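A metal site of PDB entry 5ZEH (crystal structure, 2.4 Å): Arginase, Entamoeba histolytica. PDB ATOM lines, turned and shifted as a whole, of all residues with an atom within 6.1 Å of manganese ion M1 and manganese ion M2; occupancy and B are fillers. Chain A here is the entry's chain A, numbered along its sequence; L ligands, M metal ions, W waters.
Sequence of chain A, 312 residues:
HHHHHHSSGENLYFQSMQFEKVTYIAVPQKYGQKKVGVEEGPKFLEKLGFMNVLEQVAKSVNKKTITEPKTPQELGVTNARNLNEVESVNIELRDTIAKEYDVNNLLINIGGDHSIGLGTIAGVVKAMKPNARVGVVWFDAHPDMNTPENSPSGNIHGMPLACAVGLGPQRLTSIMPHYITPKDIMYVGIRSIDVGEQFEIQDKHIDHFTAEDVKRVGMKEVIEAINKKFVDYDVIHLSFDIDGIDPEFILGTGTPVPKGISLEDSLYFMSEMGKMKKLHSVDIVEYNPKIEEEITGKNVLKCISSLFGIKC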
ATOM      1  N   HIS A 114      14.862  -4.884  22.525  1.00  0.00           N
ATOM      2  CA  HIS A 114      15.909  -3.872  22.485  1.00  0.00           C
ATOM      3  C   HIS A 114      16.884  -4.007  21.297  1.00  0.00           C
ATOM      4  O   HIS A 114      17.808  -3.221  21.191  1.00  0.00           O
ATOM      5  CB  HIS A 114      16.693  -3.838  23.805  1.00  0.00           C
ATOM      6  CG  HIS A 114      17.090  -2.456  24.227  1.00  0.00           C
ATOM      7  ND1 HIS A 114      17.423  -2.154  25.531  1.00  0.00           N
ATOM      8  CD2 HIS A 114      17.160  -1.293  23.547  1.00  0.00           C
ATOM      9  CE1 HIS A 114      17.703  -0.873  25.629  1.00  0.00           C
ATOM     10  NE2 HIS A 114      17.547  -0.323  24.436  1.00  0.00           N
ATOM     11  N   TRP A 138      21.668   4.717  28.277  1.00  0.00           N
ATOM     12  CA  TRP A 138      21.162   3.371  28.063  1.00  0.00           C
ATOM     13  C   TRP A 138      20.741   2.772  29.404  1.00  0.00           C
ATOM     14  O   TRP A 138      21.537   2.127  30.089  1.00  0.00           O
ATOM     15  CB  TRP A 138      22.215   2.541  27.358  1.00  0.00           C
ATOM     16  CG  TRP A 138      21.737   1.259  26.829  1.00  0.00           C
ATOM     17  CD1 TRP A 138      21.634   0.096  27.511  1.00  0.00           C
ATOM     18  CD2 TRP A 138      21.344   0.967  25.478  1.00  0.00           C
ATOM     19  NE1 TRP A 138      21.179  -0.908  26.679  1.00  0.00           N
ATOM     20  CE2 TRP A 138      20.996  -0.389  25.429  1.00  0.00           C
ATOM     21  CE3 TRP A 138      21.245   1.729  24.311  1.00  0.00           C
ATOM     22  CZ2 TRP A 138      20.552  -1.020  24.252  1.00  0.00           C
ATOM     23  CZ3 TRP A 138      20.793   1.097  23.140  1.00  0.00           C
ATOM     24  CH2 TRP A 138      20.459  -0.250  23.117  1.00  0.00           C
ATOM     25  N   PHE A 139      19.482   3.025  29.747  1.00  0.00           N
ATOM     26  CA  PHE A 139      18.860   2.600  31.006  1.00  0.00           C
ATOM     27  C   PHE A 139      18.360   1.179  30.807  1.00  0.00           C
ATOM     28  O   PHE A 139      17.458   0.955  29.992  1.00  0.00           O
ATOM     29  CB  PHE A 139      17.700   3.558  31.326  1.00  0.00           C
ATOM     30  CG  PHE A 139      16.980   3.273  32.602  1.00  0.00           C
ATOM     31  CD1 PHE A 139      15.974   2.304  32.643  1.00  0.00           C
ATOM     32  CD2 PHE A 139      17.251   4.001  33.754  1.00  0.00           C
ATOM     33  CE1 PHE A 139      15.292   2.056  33.806  1.00  0.00           C
ATOM     34  CE2 PHE A 139      16.563   3.758  34.929  1.00  0.00           C
ATOM     35  CZ  PHE A 139      15.575   2.778  34.958  1.00  0.00           C
ATOM     36  N   ASP A 140      18.944   0.227  31.541  1.00  0.00           N
ATOM     37  CA  ASP A 140      18.767  -1.201  31.242  1.00  0.00           C
ATOM     38  C   ASP A 140      19.371  -2.077  32.350  1.00  0.00           C
ATOM     39  O   ASP A 140      20.268  -1.635  33.054  1.00  0.00           O
ATOM     40  CB  ASP A 140      19.445  -1.520  29.887  1.00  0.00           C
ATOM     41  CG  ASP A 140      18.895  -2.758  29.209  1.00  0.00           C
ATOM     42  OD1 ASP A 140      18.606  -3.776  29.917  1.00  0.00           O
ATOM     43  OD2 ASP A 140      18.773  -2.738  27.966  1.00  0.00           O
ATOM     44  N   ALA A 141      18.868  -3.307  32.528  1.00  0.00           N
ATOM     45  CA  ALA A 141      19.547  -4.308  33.364  1.00  0.00           C
ATOM     46  C   ALA A 141      20.807  -4.881  32.677  1.00  0.00           C
ATOM     47  O   ALA A 141      21.761  -5.339  33.335  1.00  0.00           O
ATOM     48  CB  ALA A 141      18.612  -5.437  33.737  1.00  0.00           C
ATOM     49  N   HIS A 142      20.772  -4.867  31.359  1.00  0.00           N
ATOM     50  CA  HIS A 142      21.808  -5.389  30.520  1.00  0.00           C
ATOM     51  C   HIS A 142      22.566  -4.381  29.704  1.00  0.00           C
ATOM     52  O   HIS A 142      21.988  -3.432  29.237  1.00  0.00           O
ATOM     53  CB  HIS A 142      21.143  -6.261  29.494  1.00  0.00           C
ATOM     54  CG  HIS A 142      20.159  -7.222  30.068  1.00  0.00           C
ATOM     55  ND1 HIS A 142      18.812  -6.978  30.097  1.00  0.00           N
ATOM     56  CD2 HIS A 142      20.333  -8.443  30.617  1.00  0.00           C
ATOM     57  CE1 HIS A 142      18.196  -8.009  30.640  1.00  0.00           C
ATOM     58  NE2 HIS A 142      19.096  -8.910  30.953  1.00  0.00           N
ATOM     59  N   ASP A 144      23.829  -4.984  26.740  1.00  0.00           N
ATOM     60  CA  ASP A 144      23.556  -5.279  25.338  1.00  0.00           C
ATOM     61  C   ASP A 144      24.771  -5.045  24.442  1.00  0.00           C
ATOM     62  O   ASP A 144      24.675  -4.420  23.378  1.00  0.00           O
ATOM     63  CB  ASP A 144      22.360  -4.479  24.833  1.00  0.00           C
ATOM     64  CG  ASP A 144      21.089  -4.823  25.558  1.00  0.00           C
ATOM     65  OD1 ASP A 144      20.958  -5.935  26.094  1.00  0.00           O
ATOM     66  OD2 ASP A 144      20.189  -3.967  25.574  1.00  0.00           O
ATOM     67  N   HIS A 157      18.811  -8.930  20.526  1.00  0.00           N
ATOM     68  CA  HIS A 157      18.513  -7.842  21.484  1.00  0.00           C
ATOM     69  C   HIS A 157      19.571  -7.645  22.584  1.00  0.00           C
ATOM     70  O   HIS A 157      19.516  -6.646  23.314  1.00  0.00           O
ATOM     71  CB  HIS A 157      17.090  -7.968  22.057  1.00  0.00           C
ATOM     72  CG  HIS A 157      16.956  -8.905  23.221  1.00  0.00           C
ATOM     73  ND1 HIS A 157      15.952  -8.778  24.162  1.00  0.00           N
ATOM     74  CD2 HIS A 157      17.682  -9.978  23.597  1.00  0.00           C
ATOM     75  CE1 HIS A 157      16.053  -9.731  25.059  1.00  0.00           C
ATOM     76  NE2 HIS A 157      17.109 -10.474  24.740  1.00  0.00           N
ATOM     77  N   PRO A 160      22.722  -5.079  20.146  1.00  0.00           N
ATOM     78  CA  PRO A 160      22.584  -3.755  19.516  1.00  0.00           C
ATOM     79  C   PRO A 160      23.579  -2.665  19.800  1.00  0.00           C
ATOM     80  O   PRO A 160      23.930  -1.975  18.902  1.00  0.00           O
ATOM     81  CB  PRO A 160      21.224  -3.282  20.017  1.00  0.00           C
ATOM     82  CG  PRO A 160      21.086  -3.957  21.316  1.00  0.00           C
ATOM     83  CD  PRO A 160      21.557  -5.340  21.001  1.00  0.00           C
ATOM     84  N   ASP A 241      15.021   0.680  28.620  1.00  0.00           N
ATOM     85  CA  ASP A 241      14.604  -0.724  28.731  1.00  0.00           C
ATOM     86  C   ASP A 241      13.835  -0.714  30.043  1.00  0.00           C
ATOM     87  O   ASP A 241      14.354  -0.277  31.040  1.00  0.00           O
ATOM     88  CB  ASP A 241      15.849  -1.622  28.901  1.00  0.00           C
ATOM     89  CG  ASP A 241      15.630  -3.107  28.532  1.00  0.00           C
ATOM     90  OD1 ASP A 241      14.507  -3.644  28.791  1.00  0.00           O
ATOM     91  OD2 ASP A 241      16.552  -3.771  28.066  1.00  0.00           O
ATOM     92  N   ASP A 243      13.088  -3.169  31.882  1.00  0.00           N
ATOM     93  CA  ASP A 243      13.652  -4.143  32.829  1.00  0.00           C
ATOM     94  C   ASP A 243      14.871  -3.626  33.598  1.00  0.00           C
ATOM     95  O   ASP A 243      15.359  -4.308  34.489  1.00  0.00           O
ATOM     96  CB  ASP A 243      13.848  -5.532  32.214  1.00  0.00           C
ATOM     97  CG  ASP A 243      15.118  -5.680  31.425  1.00  0.00           C
ATOM     98  OD1 ASP A 243      16.238  -5.516  31.974  1.00  0.00           O
ATOM     99  OD2 ASP A 243      14.988  -6.014  30.215  1.00  0.00           O
ATOM    100  N   GLY A 244      15.340  -2.426  33.286  1.00  0.00           N
ATOM    101  CA  GLY A 244      16.224  -1.698  34.177  1.00  0.00           C
ATOM    102  C   GLY A 244      15.559  -1.410  35.510  1.00  0.00           C
ATOM    103  O   GLY A 244      16.247  -1.258  36.529  1.00  0.00           O
ATOM    104  N   THR A 255      13.135 -10.683  30.046  1.00  0.00           N
ATOM    105  CA  THR A 255      14.303 -10.956  30.868  1.00  0.00           C
ATOM    106  C   THR A 255      14.353 -10.060  32.111  1.00  0.00           C
ATOM    107  O   THR A 255      15.190  -9.171  32.206  1.00  0.00           O
ATOM    108  CB  THR A 255      15.603 -10.816  30.046  1.00  0.00           C
ATOM    109  OG1 THR A 255      15.764  -9.455  29.600  1.00  0.00           O
ATOM    110  CG2 THR A 255      15.589 -11.748  28.841  1.00  0.00           C
ATOM    111  N   VAL A 285      11.287   0.334  25.625  1.00  0.00           N
ATOM    112  CA  VAL A 285      11.461  -1.008  25.064  1.00  0.00           C
ATOM    113  C   VAL A 285      11.254  -2.167  26.043  1.00  0.00           C
ATOM    114  O   VAL A 285      11.344  -2.003  27.267  1.00  0.00           O
ATOM    115  CB  VAL A 285      12.831  -1.126  24.381  1.00  0.00           C
ATOM    116  CG1 VAL A 285      12.930  -0.209  23.168  1.00  0.00           C
ATOM    117  CG2 VAL A 285      13.992  -0.893  25.340  1.00  0.00           C
ATOM    118  N   GLU A 286      10.960  -3.332  25.476  1.00  0.00           N
ATOM    119  CA  GLU A 286      10.851  -4.630  26.184  1.00  0.00           C
ATOM    120  C   GLU A 286       9.626  -4.770  27.080  1.00  0.00           C
ATOM    121  O   GLU A 286       9.674  -5.505  28.074  1.00  0.00           O
ATOM    122  CB  GLU A 286      12.133  -4.961  27.013  1.00  0.00           C
ATOM    123  CG  GLU A 286      13.442  -5.129  26.248  1.00  0.00           C
ATOM    124  CD  GLU A 286      13.524  -6.375  25.387  1.00  0.00           C
ATOM    125  OE1 GLU A 286      12.592  -7.218  25.380  1.00  0.00           O
ATOM    126  OE2 GLU A 286      14.564  -6.499  24.683  1.00  0.00           O
HETATM  127  N1  LIG L   1      23.069 -10.872  27.750  1.00  0.00           N
HETATM  128  C1  LIG L   1      21.903 -11.722  27.453  1.00  0.00           C
HETATM  129  C2  LIG L   1      20.587 -11.018  27.810  1.00  0.00           C
HETATM  130  C3  LIG L   1      20.492  -9.620  27.170  1.00  0.00           C
HETATM  131  C4  LIG L   1      19.060  -9.114  27.290  1.00  0.00           C
HETATM  132  N2  LIG L   1      18.901  -7.797  26.661  1.00  0.00           N
HETATM  133  C5  LIG L   1      21.877 -12.183  25.986  1.00  0.00           C
HETATM  134  O1  LIG L   1      21.009 -13.026  25.696  1.00  0.00           O
HETATM  135  O2  LIG L   1      22.687 -11.689  25.179  1.00  0.00           O
HETATM  136 MN    MN M   1      17.319  -5.211  29.653  1.00  0.00          MN
HETATM  137 MN    MN M   2      18.153  -4.037  26.592  1.00  0.00          MN
HETATM  138  O   HOH W   1      17.317  -5.857  27.743  1.00  0.00           O
HETATM  139  O   HOH W   2      17.375  -6.267  25.211  1.00  0.00           O
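The side-chain carboxylate (OD1) of Asp 144 is in salt-bridge range of a nitrogen (N2) of the ligand (2.8 Å).
NE1 of Trp 138 sits close to OD2 of Asp 140. O of Phe 139 lies within hydrogen-bond range of N of Asp 241, at 2.8 Å. OD2 of Asp 144 sits close to NE1 of Trp 138. The backbone NH (N) of His 114 lies within hydrogen-bond range of the side-chain carboxylate (OE2) of Glu 286 (2.7 Å). OD1 of Asp 243 lies close to N of Ala 141 (3.5 Å).
Residues that only touch manganese ion M1: Ala 141. Within 4 Å of manganese ion M1: Asp 140, Ala 141, His 142, Asp 241 and Asp 243.
Along chain A the residues within 4 Å of manganese ion M2 span positions 114 to 241.
The side-chain carboxylate (OD1) of Asp 140 binds manganese ion M1. Manganese ion M1 is bound by water W1 (2.0 Å). OD2 of Asp 241 is bound to manganese ion M1, at 2.3 Å. Manganese ion M1 is bound by ND1 of His 142 (2.4 Å). OD2 of Asp 243 binds manganese ion M1 (2.5 Å). Manganese ion M1 is bound by OD1 of Asp 243 (2.6 Å). Manganese ion M1 has six donor atoms within binding distance.
Manganese ion M2 is bound by the side-chain carboxylate of Asp 140, the side-chain carboxylate of Asp 241, the side-chain carboxylate of Asp 144, a ring nitrogen (ND1) of His 114 and water W1. Slightly farther from manganese ion M2 lies water W2 (2.7 Å).
Water W2 lies within hydrogen-bond range of N2 of the ligand (2.6 Å), OE2 of Glu 286 (2.9 Å) and O of His 157 (2.9 Å).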
